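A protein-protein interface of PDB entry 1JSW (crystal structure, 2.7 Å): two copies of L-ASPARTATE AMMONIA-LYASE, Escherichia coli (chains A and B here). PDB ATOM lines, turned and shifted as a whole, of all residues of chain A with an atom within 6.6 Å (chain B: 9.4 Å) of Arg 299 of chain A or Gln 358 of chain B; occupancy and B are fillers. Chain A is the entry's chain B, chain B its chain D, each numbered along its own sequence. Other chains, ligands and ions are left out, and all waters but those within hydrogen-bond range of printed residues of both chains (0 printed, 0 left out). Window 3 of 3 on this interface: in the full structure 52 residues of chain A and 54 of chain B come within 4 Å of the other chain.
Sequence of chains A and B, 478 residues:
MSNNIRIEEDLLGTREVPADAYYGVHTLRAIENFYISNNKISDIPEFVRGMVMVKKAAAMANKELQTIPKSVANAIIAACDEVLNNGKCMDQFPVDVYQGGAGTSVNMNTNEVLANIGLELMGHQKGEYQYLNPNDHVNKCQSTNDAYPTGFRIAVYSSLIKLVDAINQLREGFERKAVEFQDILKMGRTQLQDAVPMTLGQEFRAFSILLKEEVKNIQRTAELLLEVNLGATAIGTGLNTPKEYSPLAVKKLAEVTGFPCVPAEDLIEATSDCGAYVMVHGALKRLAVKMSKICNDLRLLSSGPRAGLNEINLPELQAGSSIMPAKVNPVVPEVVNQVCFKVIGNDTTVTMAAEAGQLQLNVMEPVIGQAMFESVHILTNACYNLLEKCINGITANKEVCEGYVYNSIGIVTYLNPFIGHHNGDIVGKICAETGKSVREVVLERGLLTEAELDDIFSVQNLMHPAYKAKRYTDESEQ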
ATOM      1  N   SER A 292     -10.119  19.920  27.026  1.00  0.00           N
ATOM      2  CA  SER A 292      -9.413  18.670  26.840  1.00  0.00           C
ATOM      3  C   SER A 292      -9.919  18.003  25.569  1.00  0.00           C
ATOM      4  O   SER A 292      -9.159  17.831  24.612  1.00  0.00           O
ATOM      5  CB  SER A 292      -9.620  17.756  28.043  1.00  0.00           C
ATOM      6  OG  SER A 292      -8.843  16.579  27.932  1.00  0.00           O
ATOM      7  N   ILE A 294     -11.474  19.155  23.224  1.00  0.00           N
ATOM      8  CA  ILE A 294     -11.189  20.049  22.101  1.00  0.00           C
ATOM      9  C   ILE A 294      -9.777  19.732  21.630  1.00  0.00           C
ATOM     10  O   ILE A 294      -9.458  19.842  20.438  1.00  0.00           O
ATOM     11  CB  ILE A 294     -11.249  21.535  22.526  1.00  0.00           C
ATOM     12  CG1 ILE A 294     -12.678  21.940  22.867  1.00  0.00           C
ATOM     13  CG2 ILE A 294     -10.714  22.425  21.427  1.00  0.00           C
ATOM     14  CD1 ILE A 294     -12.862  23.431  23.037  1.00  0.00           C
ATOM     15  N   CYS A 295      -8.925  19.382  22.595  1.00  0.00           N
ATOM     16  CA  CYS A 295      -7.553  19.010  22.303  1.00  0.00           C
ATOM     17  C   CYS A 295      -7.526  17.549  21.925  1.00  0.00           C
ATOM     18  O   CYS A 295      -6.610  17.114  21.242  1.00  0.00           O
ATOM     19  CB  CYS A 295      -6.639  19.268  23.491  1.00  0.00           C
ATOM     20  SG  CYS A 295      -6.214  20.996  23.652  1.00  0.00           S
ATOM     21  N   ASN A 296      -8.536  16.794  22.350  1.00  0.00           N
ATOM     22  CA  ASN A 296      -8.611  15.377  22.002  1.00  0.00           C
ATOM     23  C   ASN A 296      -8.966  15.194  20.524  1.00  0.00           C
ATOM     24  O   ASN A 296      -8.459  14.282  19.872  1.00  0.00           O
ATOM     25  CB  ASN A 296      -9.612  14.647  22.892  1.00  0.00           C
ATOM     26  CG  ASN A 296      -9.095  14.451  24.306  1.00  0.00           C
ATOM     27  OD1 ASN A 296      -8.804  15.409  25.011  1.00  0.00           O
ATOM     28  ND2 ASN A 296      -8.979  13.202  24.721  1.00  0.00           N
ATOM     29  N   ASP A 297      -9.811  16.083  20.004  1.00  0.00           N
ATOM     30  CA  ASP A 297     -10.219  16.053  18.599  1.00  0.00           C
ATOM     31  C   ASP A 297      -9.047  16.392  17.701  1.00  0.00           C
ATOM     32  O   ASP A 297      -8.699  15.613  16.826  1.00  0.00           O
ATOM     33  CB  ASP A 297     -11.335  17.059  18.323  1.00  0.00           C
ATOM     34  CG  ASP A 297     -12.662  16.648  18.911  1.00  0.00           C
ATOM     35  OD1 ASP A 297     -12.687  15.812  19.851  1.00  0.00           O
ATOM     36  OD2 ASP A 297     -13.684  17.181  18.419  1.00  0.00           O
ATOM     37  N   LEU A 298      -8.445  17.561  17.917  1.00  0.00           N
ATOM     38  CA  LEU A 298      -7.296  18.006  17.121  1.00  0.00           C
ATOM     39  C   LEU A 298      -6.198  16.924  17.016  1.00  0.00           C
ATOM     40  O   LEU A 298      -5.744  16.598  15.919  1.00  0.00           O
ATOM     41  CB  LEU A 298      -6.725  19.318  17.692  1.00  0.00           C
ATOM     42  CG  LEU A 298      -7.675  20.522  17.718  1.00  0.00           C
ATOM     43  CD1 LEU A 298      -7.126  21.620  18.584  1.00  0.00           C
ATOM     44  CD2 LEU A 298      -7.933  21.033  16.316  1.00  0.00           C
ATOM     45  N   ARG A 299      -5.820  16.337  18.149  1.00  0.00           N
ATOM     46  CA  ARG A 299      -4.803  15.296  18.174  1.00  0.00           C
ATOM     47  C   ARG A 299      -5.139  14.124  17.249  1.00  0.00           C
ATOM     48  O   ARG A 299      -4.245  13.532  16.640  1.00  0.00           O
ATOM     49  CB  ARG A 299      -4.618  14.749  19.597  1.00  0.00           C
ATOM     50  CG  ARG A 299      -4.070  15.729  20.635  1.00  0.00           C
ATOM     51  CD  ARG A 299      -3.528  15.004  21.866  1.00  0.00           C
ATOM     52  NE  ARG A 299      -4.493  14.093  22.476  1.00  0.00           N
ATOM     53  CZ  ARG A 299      -4.515  12.777  22.279  1.00  0.00           C
ATOM     54  NH1 ARG A 299      -3.626  12.199  21.484  1.00  0.00           N
ATOM     55  NH2 ARG A 299      -5.417  12.030  22.897  1.00  0.00           N
ATOM     56  N   LEU A 300      -6.418  13.752  17.204  1.00  0.00           N
ATOM     57  CA  LEU A 300      -6.879  12.648  16.363  1.00  0.00           C
ATOM     58  C   LEU A 300      -7.263  13.109  14.953  1.00  0.00           C
ATOM     59  O   LEU A 300      -7.171  12.346  13.991  1.00  0.00           O
ATOM     60  CB  LEU A 300      -8.043  11.922  17.042  1.00  0.00           C
ATOM     61  CG  LEU A 300      -8.832  10.856  16.277  1.00  0.00           C
ATOM     62  CD1 LEU A 300      -7.916   9.863  15.582  1.00  0.00           C
ATOM     63  CD2 LEU A 300      -9.756  10.160  17.241  1.00  0.00           C
ATOM     64  N   LEU A 301      -7.716  14.350  14.833  1.00  0.00           N
ATOM     65  CA  LEU A 301      -8.086  14.877  13.537  1.00  0.00           C
ATOM     66  C   LEU A 301      -6.804  15.002  12.755  1.00  0.00           C
ATOM     67  O   LEU A 301      -6.799  14.866  11.529  1.00  0.00           O
ATOM     68  CB  LEU A 301      -8.728  16.255  13.663  1.00  0.00           C
ATOM     69  CG  LEU A 301     -10.133  16.328  14.241  1.00  0.00           C
ATOM     70  CD1 LEU A 301     -10.657  17.748  14.108  1.00  0.00           C
ATOM     71  CD2 LEU A 301     -11.042  15.340  13.521  1.00  0.00           C
ATOM     72  N   SER A 302      -5.723  15.283  13.480  1.00  0.00           N
ATOM     73  CA  SER A 302      -4.398  15.439  12.890  1.00  0.00           C
ATOM     74  C   SER A 302      -3.590  14.179  13.129  1.00  0.00           C
ATOM     75  O   SER A 302      -2.365  14.226  13.199  1.00  0.00           O
ATOM     76  CB  SER A 302      -3.672  16.610  13.521  1.00  0.00           C
ATOM     77  OG  SER A 302      -3.329  16.300  14.858  1.00  0.00           O
ATOM     78  N   SER A 303      -4.293  13.062  13.270  1.00  0.00           N
ATOM     79  CA  SER A 303      -3.680  11.771  13.495  1.00  0.00           C
ATOM     80  C   SER A 303      -2.689  11.372  12.412  1.00  0.00           C
ATOM     81  O   SER A 303      -2.385  12.150  11.514  1.00  0.00           O
ATOM     82  CB  SER A 303      -4.763  10.702  13.642  1.00  0.00           C
ATOM     83  OG  SER A 303      -5.731  10.782  12.610  1.00  0.00           O
ATOM     84  N   GLY A 304      -2.217  10.130  12.503  1.00  0.00           N
ATOM     85  CA  GLY A 304      -1.231   9.593  11.573  1.00  0.00           C
ATOM     86  C   GLY A 304      -1.162  10.120  10.147  1.00  0.00           C
ATOM     87  O   GLY A 304      -2.106   9.909   9.368  1.00  0.00           O
ATOM     88  N   LEU A 309      -6.539   9.924  10.189  1.00  0.00           N
ATOM     89  CA  LEU A 309      -7.347  11.111   9.913  1.00  0.00           C
ATOM     90  C   LEU A 309      -6.293  12.215   9.768  1.00  0.00           C
ATOM     91  O   LEU A 309      -5.746  12.714  10.745  1.00  0.00           O
ATOM     92  CB  LEU A 309      -8.275  11.428  11.095  1.00  0.00           C
ATOM     93  CG  LEU A 309      -9.458  10.531  11.469  1.00  0.00           C
ATOM     94  CD1 LEU A 309      -9.024   9.123  11.706  1.00  0.00           C
ATOM     95  CD2 LEU A 309     -10.117  11.068  12.711  1.00  0.00           C
ATOM     96  N   ILE A 312      -6.187  17.779   9.504  1.00  0.00           N
ATOM     97  CA  ILE A 312      -5.525  19.049   9.775  1.00  0.00           C
ATOM     98  C   ILE A 312      -4.025  18.895   9.974  1.00  0.00           C
ATOM     99  O   ILE A 312      -3.466  17.834   9.701  1.00  0.00           O
ATOM    100  CB  ILE A 312      -6.162  19.774  10.977  1.00  0.00           C
ATOM    101  CG1 ILE A 312      -6.132  18.889  12.217  1.00  0.00           C
ATOM    102  CG2 ILE A 312      -7.597  20.160  10.659  1.00  0.00           C
ATOM    103  CD1 ILE A 312      -6.769  19.542  13.405  1.00  0.00           C
ATOM    104  N   LEU A 314      -1.096  20.274  12.917  1.00  0.00           N
ATOM    105  CA  LEU A 314      -0.649  21.066  14.054  1.00  0.00           C
ATOM    106  C   LEU A 314       0.800  21.442  13.769  1.00  0.00           C
ATOM    107  O   LEU A 314       1.534  20.651  13.187  1.00  0.00           O
ATOM    108  CB  LEU A 314      -0.756  20.286  15.375  1.00  0.00           C
ATOM    109  CG  LEU A 314      -2.107  20.144  16.096  1.00  0.00           C
ATOM    110  CD1 LEU A 314      -2.908  21.425  16.023  1.00  0.00           C
ATOM    111  CD2 LEU A 314      -2.900  19.048  15.474  1.00  0.00           C
ATOM    112  N   PRO A 330       1.392  15.718  18.102  1.00  0.00           N
ATOM    113  CA  PRO A 330       0.307  16.597  18.569  1.00  0.00           C
ATOM    114  C   PRO A 330       0.685  17.040  19.971  1.00  0.00           C
ATOM    115  O   PRO A 330      -0.024  16.792  20.940  1.00  0.00           O
ATOM    116  CB  PRO A 330      -0.887  15.656  18.593  1.00  0.00           C
ATOM    117  CG  PRO A 330      -0.254  14.344  18.979  1.00  0.00           C
ATOM    118  CD  PRO A 330       0.955  14.311  18.088  1.00  0.00           C
ATOM    119  N   VAL A 331       1.813  17.732  20.040  1.00  0.00           N
ATOM    120  CA  VAL A 331       2.410  18.172  21.284  1.00  0.00           C
ATOM    121  C   VAL A 331       1.695  19.233  22.116  1.00  0.00           C
ATOM    122  O   VAL A 331       1.425  18.993  23.295  1.00  0.00           O
ATOM    123  CB  VAL A 331       3.891  18.534  21.026  1.00  0.00           C
ATOM    124  CG1 VAL A 331       4.082  20.033  20.862  1.00  0.00           C
ATOM    125  CG2 VAL A 331       4.761  17.947  22.081  1.00  0.00           C
ATOM    126  N   PRO A 333      -1.462  20.203  22.229  1.00  0.00           N
ATOM    127  CA  PRO A 333      -2.718  19.793  22.861  1.00  0.00           C
ATOM    128  C   PRO A 333      -2.480  18.837  24.026  1.00  0.00           C
ATOM    129  O   PRO A 333      -3.157  18.913  25.049  1.00  0.00           O
ATOM    130  CB  PRO A 333      -3.456  19.110  21.716  1.00  0.00           C
ATOM    131  CG  PRO A 333      -2.977  19.880  20.532  1.00  0.00           C
ATOM    132  CD  PRO A 333      -1.503  19.928  20.788  1.00  0.00           C
ATOM    133  N   GLU A 334      -1.498  17.958  23.872  1.00  0.00           N
ATOM    134  CA  GLU A 334      -1.183  17.003  24.915  1.00  0.00           C
ATOM    135  C   GLU A 334      -0.933  17.702  26.236  1.00  0.00           C
ATOM    136  O   GLU A 334      -1.592  17.418  27.230  1.00  0.00           O
ATOM    137  CB  GLU A 334       0.034  16.163  24.534  1.00  0.00           C
ATOM    138  CG  GLU A 334      -0.233  15.184  23.415  1.00  0.00           C
ATOM    139  CD  GLU A 334       1.007  14.462  22.926  1.00  0.00           C
ATOM    140  OE1 GLU A 334       2.127  14.763  23.390  1.00  0.00           O
ATOM    141  OE2 GLU A 334       0.855  13.574  22.069  1.00  0.00           O
ATOM    142  N   ASN A 337      -3.995  18.713  27.708  1.00  0.00           N
ATOM    143  CA  ASN A 337      -4.776  17.622  28.272  1.00  0.00           C
ATOM    144  C   ASN A 337      -4.259  17.418  29.677  1.00  0.00           C
ATOM    145  O   ASN A 337      -5.019  17.183  30.604  1.00  0.00           O
ATOM    146  CB  ASN A 337      -4.578  16.330  27.480  1.00  0.00           C
ATOM    147  CG  ASN A 337      -5.088  16.425  26.055  1.00  0.00           C
ATOM    148  OD1 ASN A 337      -4.315  16.655  25.129  1.00  0.00           O
ATOM    149  ND2 ASN A 337      -6.392  16.232  25.872  1.00  0.00           N
ATOM    150  N   GLY B 100       4.229  18.120  26.451  1.00  0.00           N
ATOM    151  CA  GLY B 100       3.833  17.107  25.501  1.00  0.00           C
ATOM    152  C   GLY B 100       5.057  16.344  25.073  1.00  0.00           C
ATOM    153  O   GLY B 100       6.090  16.365  25.749  1.00  0.00           O
ATOM    154  N   GLY B 101       4.958  15.687  23.928  1.00  0.00           N
ATOM    155  CA  GLY B 101       6.083  14.916  23.440  1.00  0.00           C
ATOM    156  C   GLY B 101       6.291  13.690  24.301  1.00  0.00           C
ATOM    157  O   GLY B 101       7.132  12.867  23.984  1.00  0.00           O
ATOM    158  N   ILE B 235       7.058  -0.003  18.668  1.00  0.00           N
ATOM    159  CA  ILE B 235       5.643  -0.176  18.361  1.00  0.00           C
ATOM    160  C   ILE B 235       5.040  -1.411  19.042  1.00  0.00           C
ATOM    161  O   ILE B 235       4.340  -1.277  20.045  1.00  0.00           O
ATOM    162  CB  ILE B 235       5.364  -0.195  16.827  1.00  0.00           C
ATOM    163  CG1 ILE B 235       6.559  -0.759  16.040  1.00  0.00           C
ATOM    164  CG2 ILE B 235       5.018   1.212  16.346  1.00  0.00           C
ATOM    165  CD1 ILE B 235       6.669  -2.266  15.969  1.00  0.00           C
ATOM    166  N   GLU B 269       3.502  -2.497  25.429  1.00  0.00           N
ATOM    167  CA  GLU B 269       2.407  -1.744  26.048  1.00  0.00           C
ATOM    168  C   GLU B 269       2.828  -1.059  27.335  1.00  0.00           C
ATOM    169  O   GLU B 269       2.165  -0.137  27.795  1.00  0.00           O
ATOM    170  CB  GLU B 269       1.172  -2.642  26.270  1.00  0.00           C
ATOM    171  CG  GLU B 269       0.105  -2.149  27.290  1.00  0.00           C
ATOM    172  CD  GLU B 269      -0.770  -0.971  26.812  1.00  0.00           C
ATOM    173  OE1 GLU B 269      -1.113  -0.899  25.609  1.00  0.00           O
ATOM    174  OE2 GLU B 269      -1.144  -0.131  27.666  1.00  0.00           O
ATOM    175  N   THR B 271       5.291   0.927  27.794  1.00  0.00           N
ATOM    176  CA  THR B 271       5.557   2.323  27.403  1.00  0.00           C
ATOM    177  C   THR B 271       4.220   2.974  27.019  1.00  0.00           C
ATOM    178  O   THR B 271       4.009   4.176  27.233  1.00  0.00           O
ATOM    179  CB  THR B 271       6.533   2.403  26.174  1.00  0.00           C
ATOM    180  OG1 THR B 271       7.011   3.743  26.013  1.00  0.00           O
ATOM    181  CG2 THR B 271       5.824   1.982  24.869  1.00  0.00           C
ATOM    182  N   SER B 272       3.322   2.145  26.474  1.00  0.00           N
ATOM    183  CA  SER B 272       1.980   2.545  26.034  1.00  0.00           C
ATOM    184  C   SER B 272       1.055   2.745  27.240  1.00  0.00           C
ATOM    185  O   SER B 272      -0.155   2.955  27.066  1.00  0.00           O
ATOM    186  CB  SER B 272       1.393   1.456  25.130  1.00  0.00           C
ATOM    187  OG  SER B 272       2.407   0.792  24.377  1.00  0.00           O
ATOM    188  N   ASP B 273       1.649   2.604  28.439  1.00  0.00           N
ATOM    189  CA  ASP B 273       1.036   2.744  29.777  1.00  0.00           C
ATOM    190  C   ASP B 273       1.286   1.559  30.725  1.00  0.00           C
ATOM    191  O   ASP B 273       0.716   0.463  30.545  1.00  0.00           O
ATOM    192  CB  ASP B 273      -0.485   3.015  29.724  1.00  0.00           C
ATOM    193  CG  ASP B 273      -1.105   3.239  31.110  1.00  0.00           C
ATOM    194  OD1 ASP B 273      -0.380   3.470  32.101  1.00  0.00           O
ATOM    195  OD2 ASP B 273      -2.341   3.169  31.219  1.00  0.00           O
ATOM    196  N   MET B 352      -7.053   9.759  35.201  1.00  0.00           N
ATOM    197  CA  MET B 352      -7.452  10.341  33.926  1.00  0.00           C
ATOM    198  C   MET B 352      -6.363  10.231  32.887  1.00  0.00           C
ATOM    199  O   MET B 352      -6.630   9.979  31.715  1.00  0.00           O
ATOM    200  CB  MET B 352      -7.804  11.801  34.104  1.00  0.00           C
ATOM    201  CG  MET B 352      -9.139  12.014  34.714  1.00  0.00           C
ATOM    202  SD  MET B 352     -10.008  13.169  33.694  1.00  0.00           S
ATOM    203  CE  MET B 352     -10.821  12.066  32.469  1.00  0.00           C
ATOM    204  N   ALA B 353      -5.137  10.485  33.317  1.00  0.00           N
ATOM    205  CA  ALA B 353      -3.986  10.391  32.445  1.00  0.00           C
ATOM    206  C   ALA B 353      -3.766   8.933  32.075  1.00  0.00           C
ATOM    207  O   ALA B 353      -3.545   8.614  30.916  1.00  0.00           O
ATOM    208  CB  ALA B 353      -2.766  10.940  33.144  1.00  0.00           C
ATOM    209  N   ALA B 354      -3.862   8.049  33.063  1.00  0.00           N
ATOM    210  CA  ALA B 354      -3.656   6.624  32.842  1.00  0.00           C
ATOM    211  C   ALA B 354      -4.707   6.057  31.917  1.00  0.00           C
ATOM    212  O   ALA B 354      -4.576   4.945  31.417  1.00  0.00           O
ATOM    213  CB  ALA B 354      -3.662   5.877  34.160  1.00  0.00           C
ATOM    214  N   GLU B 355      -5.760   6.826  31.705  1.00  0.00           N
ATOM    215  CA  GLU B 355      -6.842   6.411  30.835  1.00  0.00           C
ATOM    216  C   GLU B 355      -6.546   6.935  29.432  1.00  0.00           C
ATOM    217  O   GLU B 355      -6.890   6.301  28.432  1.00  0.00           O
ATOM    218  CB  GLU B 355      -8.151   6.991  31.369  1.00  0.00           C
ATOM    219  CG  GLU B 355      -9.402   6.341  30.850  1.00  0.00           C
ATOM    220  CD  GLU B 355      -9.897   6.949  29.567  1.00  0.00           C
ATOM    221  OE1 GLU B 355      -9.564   8.124  29.275  1.00  0.00           O
ATOM    222  OE2 GLU B 355     -10.646   6.249  28.858  1.00  0.00           O
ATOM    223  N   ALA B 356      -5.830   8.055  29.380  1.00  0.00           N
ATOM    224  CA  ALA B 356      -5.476   8.714  28.133  1.00  0.00           C
ATOM    225  C   ALA B 356      -4.429   8.028  27.269  1.00  0.00           C
ATOM    226  O   ALA B 356      -3.771   8.674  26.453  1.00  0.00           O
ATOM    227  CB  ALA B 356      -5.054  10.124  28.415  1.00  0.00           C
ATOM    228  N   GLY B 357      -4.256   6.728  27.453  1.00  0.00           N
ATOM    229  CA  GLY B 357      -3.301   6.009  26.641  1.00  0.00           C
ATOM    230  C   GLY B 357      -3.904   5.747  25.274  1.00  0.00           C
ATOM    231  O   GLY B 357      -5.086   5.441  25.177  1.00  0.00           O
ATOM    232  N   GLN B 358      -3.112   5.894  24.218  1.00  0.00           N
ATOM    233  CA  GLN B 358      -3.598   5.659  22.867  1.00  0.00           C
ATOM    234  C   GLN B 358      -2.732   4.703  22.057  1.00  0.00           C
ATOM    235  O   GLN B 358      -1.593   5.009  21.712  1.00  0.00           O
ATOM    236  CB  GLN B 358      -3.773   6.977  22.110  1.00  0.00           C
ATOM    237  CG  GLN B 358      -5.065   7.716  22.439  1.00  0.00           C
ATOM    238  CD  GLN B 358      -5.336   8.859  21.486  1.00  0.00           C
ATOM    239  OE1 GLN B 358      -4.414   9.558  21.076  1.00  0.00           O
ATOM    240  NE2 GLN B 358      -6.605   9.057  21.126  1.00  0.00           N
ATOM    241  N   LEU B 359      -3.300   3.542  21.756  1.00  0.00           N
ATOM    242  CA  LEU B 359      -2.641   2.500  20.975  1.00  0.00           C
ATOM    243  C   LEU B 359      -1.288   2.063  21.530  1.00  0.00           C
ATOM    244  O   LEU B 359      -1.214   1.590  22.669  1.00  0.00           O
ATOM    245  CB  LEU B 359      -2.548   2.908  19.494  1.00  0.00           C
ATOM    246  CG  LEU B 359      -3.875   3.069  18.715  1.00  0.00           C
ATOM    247  CD1 LEU B 359      -3.616   3.297  17.233  1.00  0.00           C
ATOM    248  CD2 LEU B 359      -4.747   1.834  18.881  1.00  0.00           C
ATOM    249  N   GLN B 360      -0.228   2.217  20.736  1.00  0.00           N
ATOM    250  CA  GLN B 360       1.123   1.818  21.144  1.00  0.00           C
ATOM    251  C   GLN B 360       1.913   2.745  22.071  1.00  0.00           C
ATOM    252  O   GLN B 360       3.054   2.426  22.405  1.00  0.00           O
ATOM    253  CB  GLN B 360       1.988   1.453  19.929  1.00  0.00           C
ATOM    254  CG  GLN B 360       1.450   1.893  18.574  1.00  0.00           C
ATOM    255  CD  GLN B 360       0.459   0.905  17.965  1.00  0.00           C
ATOM    256  OE1 GLN B 360       0.089   1.025  16.795  1.00  0.00           O
ATOM    257  NE2 GLN B 360       0.024  -0.072  18.757  1.00  0.00           N
ATOM    258  N   LEU B 361       1.320   3.863  22.503  1.00  0.00           N
ATOM    259  CA  LEU B 361       1.999   4.790  23.423  1.00  0.00           C
ATOM    260  C   LEU B 361       1.152   5.829  24.169  1.00  0.00           C
ATOM    261  O   LEU B 361       0.444   6.646  23.563  1.00  0.00           O
ATOM    262  CB  LEU B 361       3.168   5.520  22.747  1.00  0.00           C
ATOM    263  CG  LEU B 361       3.844   6.574  23.634  1.00  0.00           C
ATOM    264  CD1 LEU B 361       4.487   5.907  24.819  1.00  0.00           C
ATOM    265  CD2 LEU B 361       4.864   7.357  22.868  1.00  0.00           C
ATOM    266  N   ASN B 362       1.335   5.830  25.491  1.00  0.00           N
ATOM    267  CA  ASN B 362       0.678   6.754  26.417  1.00  0.00           C
ATOM    268  C   ASN B 362       1.587   7.981  26.459  1.00  0.00           C
ATOM    269  O   ASN B 362       2.809   7.842  26.573  1.00  0.00           O
ATOM    270  CB  ASN B 362       0.607   6.127  27.815  1.00  0.00           C
ATOM    271  CG  ASN B 362      -0.546   6.660  28.635  1.00  0.00           C
ATOM    272  OD1 ASN B 362      -0.774   7.865  28.700  1.00  0.00           O
ATOM    273  ND2 ASN B 362      -1.298   5.760  29.246  1.00  0.00           N
ATOM    274  N   VAL B 363       1.013   9.172  26.354  1.00  0.00           N
ATOM    275  CA  VAL B 363       1.828  10.381  26.353  1.00  0.00           C
ATOM    276  C   VAL B 363       1.614  11.223  27.597  1.00  0.00           C
ATOM    277  O   VAL B 363       2.233  12.279  27.759  1.00  0.00           O
ATOM    278  CB  VAL B 363       1.543  11.257  25.102  1.00  0.00           C
ATOM    279  CG1 VAL B 363       1.386  10.391  23.868  1.00  0.00           C
ATOM    280  CG2 VAL B 363       0.300  12.100  25.296  1.00  0.00           C
ATOM    281  N   MET B 364       0.738  10.751  28.473  1.00  0.00           N
ATOM    282  CA  MET B 364       0.423  11.483  29.681  1.00  0.00           C
ATOM    283  C   MET B 364       1.274  11.052  30.865  1.00  0.00           C
ATOM    284  O   MET B 364       0.890  11.235  32.016  1.00  0.00           O
ATOM    285  CB  MET B 364      -1.065  11.350  29.997  1.00  0.00           C
ATOM    286  CG  MET B 364      -2.005  11.651  28.823  1.00  0.00           C
ATOM    287  SD  MET B 364      -2.058  13.372  28.254  1.00  0.00           S
ATOM    288  CE  MET B 364      -2.838  13.206  26.674  1.00  0.00           C
ATOM    289  N   GLU B 365       2.423  10.448  30.588  1.00  0.00           N
ATOM    290  CA  GLU B 365       3.331  10.044  31.660  1.00  0.00           C
ATOM    291  C   GLU B 365       3.821  11.291  32.428  1.00  0.00           C
ATOM    292  O   GLU B 365       3.806  11.308  33.664  1.00  0.00           O
ATOM    293  CB  GLU B 365       4.533   9.253  31.107  1.00  0.00           C
ATOM    294  CG  GLU B 365       4.244   7.815  30.683  1.00  0.00           C
ATOM    295  CD  GLU B 365       4.886   7.437  29.344  1.00  0.00           C
ATOM    296  OE1 GLU B 365       5.845   8.104  28.904  1.00  0.00           O
ATOM    297  OE2 GLU B 365       4.412   6.470  28.712  1.00  0.00           O
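No position is printed for both chains.
Of the 7 pairs that touch across the chains among the printed residues, none has its exchanged pair printed and touching as well.
OE1 of Glu 334 of chain A sits at hydrogen-bond distance from N of Gly 101 of chain B.
The side-chain amide oxygen (OE1) of Gln 358 of chain B is in hydrogen-bond range of the guanidinium group (NH1) of Arg 299 of chain A (2.8 Å).
OG of Ser 302 of chain A lies within hydrogen-bond range of O of Arg 299 of chain A (3.4 Å).
O of Pro 333 of chain A lies close to OD1 of Asn 337 of chain A.
The side-chain hydroxyl (OG) of Ser 292 of chain A lies within hydrogen-bond range of the side-chain amide nitrogen (ND2) of Asn 337 of chain A.
OD1 of Asn 362 of chain B sits at hydrogen-bond distance from N of Met 364 of chain B (3.3 Å).
N of Glu 334 of chain A sits close to OD1 of Asn 337 of chain A.
OD1 of Asn 296 of chain A is in hydrogen-bond range of ND2 of Asn 337 of chain A, at 2.7 Å.
Among the printed residues, merely in contact across the chains: Val 331 of chain A with Gly 101 of chain B (2.9 Å), Val 331 of chain A with Gly 100 of chain B (3.4 Å), Glu 334 of chain A with Val 363 of chain B (3.4 Å), Glu 334 of chain A with Gly 100 of chain B (3.6 Å) and Asn 337 of chain A with Met 364 of chain B (3.7 Å).
No residue of chain B comes within 4 Å of Asn 296 of chain A.
Leu 298 of chain A touches none of the printed residues of chain B.
Arg 299 of chain A touches just one residue of chain B: Gln 358 (2.8 Å).
No residue of chain B comes within 4 Å of Ser 302 of chain A.
Of the printed residues of chain A, Gly 101 of chain B touches Val 331 and Glu 334.
Glu 355 of chain B touches none of the printed residues of chain A.
Gln 358 of chain B touches just one residue of chain A: Arg 299.
Of the printed residues of chain A, Met 364 of chain B touches Asn 337 (3.7 Å).
The nearest residue of chain A that does not touch Gln 358 of chain B is Leu 300 of chain A (5.1 Å).
The nearest printed residue of chain A that does not touch Val 363 of chain B is Arg 299 of chain A (5.5 Å).
Printed residues of chain B that touch a printed residue of chain A: Gly 100, Gly 101, Gln 358, Val 363 and Met 364.
Among the printed residues, 7 pairs touch across the chains.
Among the printed residues, no Asp or Glu carboxylate lies within 4 Å of a Lys or Arg side-chain nitrogen of the other chain.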
